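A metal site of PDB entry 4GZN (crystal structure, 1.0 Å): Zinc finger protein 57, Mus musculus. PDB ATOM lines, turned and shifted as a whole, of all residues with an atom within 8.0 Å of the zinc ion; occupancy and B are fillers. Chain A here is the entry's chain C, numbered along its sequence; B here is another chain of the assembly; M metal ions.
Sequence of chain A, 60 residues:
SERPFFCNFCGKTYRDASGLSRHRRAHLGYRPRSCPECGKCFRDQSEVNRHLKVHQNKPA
The backbone NH (N) of Cys 35 lies within hydrogen-bond range of the backbone carbonyl oxygen (O) of Lys 40, at 2.8 Å. ND1 of His 55 lies close to OE1 of Glu 37 (3.4 Å). SG of Cys 38 sits close to N of Lys 40 (3.5 Å). The backbone NH of Glu 37 lies close to the side-chain sulfur of Cys 35, at 3.4 Å. OP2 of DT 3 of chain B lies within hydrogen-bond range of a ring nitrogen (ND1) of His 51.
Four residues have an atom within 4 Å of the zinc ion: Cys 35, Cys 38, His 51 and His 55. The nearest printed residue that does not touch the zinc ion is Glu 37 (4.4 Å).
The zinc ion is bound by NE2 of His 55 (2.0 Å), NE2 of His 51 (2.1 Å), SG of Cys 38 (2.3 Å) and SG of Cys 35 (2.3 Å).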
ATOM      1  N   SER A  34      10.344  -0.785   9.744  1.00  0.00           N
ATOM      2  CA  SER A  34      10.062  -0.870   8.327  1.00  0.00           C
ATOM      3  C   SER A  34       9.975   0.486   7.645  1.00  0.00           C
ATOM      4  O   SER A  34       9.634   1.498   8.258  1.00  0.00           O
ATOM      5  CB  SER A  34       8.788  -1.654   8.092  1.00  0.00           C
ATOM      6  OG  SER A  34       7.728  -1.037   8.780  1.00  0.00           O
ATOM      7  N   CYS A  35      10.283   0.479   6.370  1.00  0.00           N
ATOM      8  CA  CYS A  35      10.078   1.648   5.544  1.00  0.00           C
ATOM      9  C   CYS A  35       8.574   1.895   5.390  1.00  0.00           C
ATOM     10  O   CYS A  35       7.845   1.012   4.956  1.00  0.00           O
ATOM     11  CB  CYS A  35      10.675   1.402   4.180  1.00  0.00           C
ATOM     12  SG  CYS A  35      10.403   2.801   3.056  1.00  0.00           S
ATOM     13  N   PRO A  36       8.110   3.109   5.728  1.00  0.00           N
ATOM     14  CA  PRO A  36       6.662   3.355   5.605  1.00  0.00           C
ATOM     15  C   PRO A  36       6.227   3.463   4.147  1.00  0.00           C
ATOM     16  O   PRO A  36       5.045   3.300   3.835  1.00  0.00           O
ATOM     17  CB  PRO A  36       6.475   4.689   6.337  1.00  0.00           C
ATOM     18  CG  PRO A  36       7.790   5.365   6.238  1.00  0.00           C
ATOM     19  CD  PRO A  36       8.823   4.258   6.309  1.00  0.00           C
ATOM     20  N   GLU A  37       7.166   3.731   3.258  1.00  0.00           N
ATOM     21  CA  GLU A  37       6.807   3.840   1.864  1.00  0.00           C
ATOM     22  C   GLU A  37       6.574   2.463   1.217  1.00  0.00           C
ATOM     23  O   GLU A  37       5.522   2.232   0.617  1.00  0.00           O
ATOM     24  CB  GLU A  37       7.880   4.642   1.124  1.00  0.00           C
ATOM     25  CG  GLU A  37       7.368   5.345  -0.097  1.00  0.00           C
ATOM     26  CD  GLU A  37       6.848   4.369  -1.113  1.00  0.00           C
ATOM     27  OE1 GLU A  37       7.537   3.348  -1.348  1.00  0.00           O
ATOM     28  OE2 GLU A  37       5.756   4.607  -1.651  1.00  0.00           O
ATOM     29  N   CYS A  38       7.531   1.540   1.377  1.00  0.00           N
ATOM     30  CA  CYS A  38       7.495   0.258   0.659  1.00  0.00           C
ATOM     31  C   CYS A  38       7.355  -0.974   1.534  1.00  0.00           C
ATOM     32  O   CYS A  38       7.147  -2.071   1.019  1.00  0.00           O
ATOM     33  CB  CYS A  38       8.716   0.101  -0.263  1.00  0.00           C
ATOM     34  SG  CYS A  38      10.276  -0.220   0.631  1.00  0.00           S
ATOM     35  N   GLY A  39       7.478  -0.808   2.843  1.00  0.00           N
ATOM     36  CA  GLY A  39       7.325  -1.931   3.754  1.00  0.00           C
ATOM     37  C   GLY A  39       8.581  -2.744   4.017  1.00  0.00           C
ATOM     38  O   GLY A  39       8.575  -3.635   4.847  1.00  0.00           O
ATOM     39  N   LYS A  40       9.674  -2.450   3.318  1.00  0.00           N
ATOM     40  CA  LYS A  40      10.891  -3.230   3.527  1.00  0.00           C
ATOM     41  C   LYS A  40      11.391  -3.061   4.957  1.00  0.00           C
ATOM     42  O   LYS A  40      11.429  -1.943   5.500  1.00  0.00           O
ATOM     43  CB  LYS A  40      11.968  -2.845   2.526  1.00  0.00           C
ATOM     44  CG  LYS A  40      13.161  -3.768   2.567  1.00  0.00           C
ATOM     45  CD  LYS A  40      14.049  -3.577   1.354  1.00  0.00           C
ATOM     46  CE  LYS A  40      15.236  -4.511   1.403  1.00  0.00           C
ATOM     47  NZ  LYS A  40      16.025  -4.494   0.135  1.00  0.00           N
ATOM     48  N   CYS A  41      11.781  -4.172   5.569  1.00  0.00           N
ATOM     49  CA  CYS A  41      12.198  -4.185   6.970  1.00  0.00           C
ATOM     50  C   CYS A  41      13.703  -4.095   7.129  1.00  0.00           C
ATOM     51  O   CYS A  41      14.461  -4.628   6.315  1.00  0.00           O
ATOM     52  CB  CYS A  41      11.671  -5.433   7.659  1.00  0.00           C
ATOM     53  SG  CYS A  41       9.866  -5.474   7.717  1.00  0.00           S
ATOM     54  N   PHE A  42      14.109  -3.441   8.220  1.00  0.00           N
ATOM     55  CA  PHE A  42      15.505  -3.226   8.563  1.00  0.00           C
ATOM     56  C   PHE A  42      15.705  -3.400  10.060  1.00  0.00           C
ATOM     57  O   PHE A  42      14.759  -3.451  10.844  1.00  0.00           O
ATOM     58  CB  PHE A  42      15.967  -1.819   8.126  1.00  0.00           C
ATOM     59  CG  PHE A  42      16.048  -1.641   6.633  1.00  0.00           C
ATOM     60  CD1 PHE A  42      17.211  -1.950   5.949  1.00  0.00           C
ATOM     61  CD2 PHE A  42      14.953  -1.183   5.918  1.00  0.00           C
ATOM     62  CE1 PHE A  42      17.296  -1.817   4.584  1.00  0.00           C
ATOM     63  CE2 PHE A  42      15.033  -1.040   4.536  1.00  0.00           C
ATOM     64  CZ  PHE A  42      16.198  -1.358   3.883  1.00  0.00           C
ATOM     65  N   VAL A  48      16.481   2.170   8.233  1.00  0.00           N
ATOM     66  CA  VAL A  48      15.322   2.608   7.452  1.00  0.00           C
ATOM     67  C   VAL A  48      15.598   3.998   6.841  1.00  0.00           C
ATOM     68  O   VAL A  48      15.384   4.222   5.646  1.00  0.00           O
ATOM     69  CB  VAL A  48      14.036   2.692   8.299  1.00  0.00           C
ATOM     70  CG1 VAL A  48      12.911   3.323   7.494  1.00  0.00           C
ATOM     71  CG2 VAL A  48      13.619   1.300   8.792  1.00  0.00           C
ATOM     72  N   HIS A  51      17.800   4.010   3.886  1.00  0.00           N
ATOM     73  CA  HIS A  51      17.103   3.391   2.756  1.00  0.00           C
ATOM     74  C   HIS A  51      16.151   4.356   2.036  1.00  0.00           C
ATOM     75  O   HIS A  51      15.906   4.180   0.831  1.00  0.00           O
ATOM     76  CB  HIS A  51      16.334   2.177   3.270  1.00  0.00           C
ATOM     77  CG  HIS A  51      15.175   1.780   2.404  1.00  0.00           C
ATOM     78  ND1 HIS A  51      15.304   1.019   1.257  1.00  0.00           N
ATOM     79  CD2 HIS A  51      13.857   2.066   2.522  1.00  0.00           C
ATOM     80  CE1 HIS A  51      14.098   0.874   0.708  1.00  0.00           C
ATOM     81  NE2 HIS A  51      13.205   1.497   1.459  1.00  0.00           N
ATOM     82  N   LEU A  52      15.589   5.329   2.739  1.00  0.00           N
ATOM     83  CA  LEU A  52      14.476   6.108   2.193  1.00  0.00           C
ATOM     84  C   LEU A  52      14.785   6.732   0.839  1.00  0.00           C
ATOM     85  O   LEU A  52      13.879   6.869   0.012  1.00  0.00           O
ATOM     86  CB  LEU A  52      14.037   7.203   3.155  1.00  0.00           C
ATOM     87  CG  LEU A  52      13.532   6.756   4.521  1.00  0.00           C
ATOM     88  CD1 LEU A  52      13.340   7.960   5.404  1.00  0.00           C
ATOM     89  CD2 LEU A  52      12.259   5.936   4.384  1.00  0.00           C
ATOM     90  N   LYS A  53      16.035   7.134   0.623  1.00  0.00           N
ATOM     91  CA  LYS A  53      16.394   7.831  -0.616  1.00  0.00           C
ATOM     92  C   LYS A  53      16.146   7.005  -1.863  1.00  0.00           C
ATOM     93  O   LYS A  53      16.081   7.561  -2.955  1.00  0.00           O
ATOM     94  CB  LYS A  53      17.823   8.362  -0.585  1.00  0.00           C
ATOM     95  CG  LYS A  53      18.875   7.282  -0.514  1.00  0.00           C
ATOM     96  CD  LYS A  53      20.287   7.849  -0.541  1.00  0.00           C
ATOM     97  CE  LYS A  53      20.641   8.617   0.723  1.00  0.00           C
ATOM     98  NZ  LYS A  53      20.755   7.756   1.939  1.00  0.00           N
ATOM     99  N   VAL A  54      15.981   5.685  -1.740  1.00  0.00           N
ATOM    100  CA  VAL A  54      15.526   4.847  -2.847  1.00  0.00           C
ATOM    101  C   VAL A  54      14.294   5.458  -3.523  1.00  0.00           C
ATOM    102  O   VAL A  54      14.084   5.321  -4.727  1.00  0.00           O
ATOM    103  CB  VAL A  54      15.174   3.409  -2.366  1.00  0.00           C
ATOM    104  CG1 VAL A  54      14.387   2.636  -3.408  1.00  0.00           C
ATOM    105  CG2 VAL A  54      16.433   2.649  -1.986  1.00  0.00           C
ATOM    106  N   HIS A  55      13.447   6.096  -2.715  1.00  0.00           N
ATOM    107  CA  HIS A  55      12.156   6.581  -3.185  1.00  0.00           C
ATOM    108  C   HIS A  55      12.166   7.989  -3.742  1.00  0.00           C
ATOM    109  O   HIS A  55      11.119   8.492  -4.151  1.00  0.00           O
ATOM    110  CB  HIS A  55      11.112   6.430  -2.082  1.00  0.00           C
ATOM    111  CG  HIS A  55      11.005   5.030  -1.565  1.00  0.00           C
ATOM    112  ND1 HIS A  55      10.741   3.958  -2.389  1.00  0.00           N
ATOM    113  CD2 HIS A  55      11.209   4.514  -0.331  1.00  0.00           C
ATOM    114  CE1 HIS A  55      10.763   2.849  -1.666  1.00  0.00           C
ATOM    115  NE2 HIS A  55      11.040   3.156  -0.413  1.00  0.00           N
ATOM    116  P    DT B   3      18.065  -1.103  -0.232  1.00  0.00           P
ATOM    117  OP1  DT B   3      16.884  -1.997  -0.345  1.00  0.00           O
ATOM    118  OP2  DT B   3      17.859   0.217   0.412  1.00  0.00           O
ATOM    119  O5'  DT B   3      19.227  -1.844   0.541  1.00  0.00           O
ATOM    120  C5'  DT B   3      19.682  -3.125   0.116  1.00  0.00           C
ATOM    121  C4'  DT B   3      20.897  -3.469   0.939  1.00  0.00           C
ATOM    122  O4'  DT B   3      22.003  -2.622   0.547  1.00  0.00           O
ATOM    123  C3'  DT B   3      20.724  -3.296   2.449  1.00  0.00           C
ATOM    124  O3'  DT B   3      21.327  -4.362   3.136  1.00  0.00           O
ATOM    125  C2'  DT B   3      21.558  -2.050   2.751  1.00  0.00           C
ATOM    126  C1'  DT B   3      22.672  -2.290   1.748  1.00  0.00           C
ATOM    127  N1   DT B   3      23.582  -1.155   1.520  1.00  0.00           N
ATOM    128  C2   DT B   3      24.932  -1.433   1.385  1.00  0.00           C
ATOM    129  O2   DT B   3      25.389  -2.562   1.419  1.00  0.00           O
ATOM    130  N3   DT B   3      25.725  -0.346   1.186  1.00  0.00           N
ATOM    131  C4   DT B   3      25.334   0.966   1.113  1.00  0.00           C
ATOM    132  O4   DT B   3      26.151   1.858   0.955  1.00  0.00           O
ATOM    133  C5   DT B   3      23.905   1.197   1.255  1.00  0.00           C
ATOM    134  C7   DT B   3      23.373   2.597   1.206  1.00  0.00           C
ATOM    135  C6   DT B   3      23.106   0.139   1.450  1.00  0.00           C
HETATM  136 ZN    ZN M   1      11.206   1.825   1.125  1.00  0.00          ZN
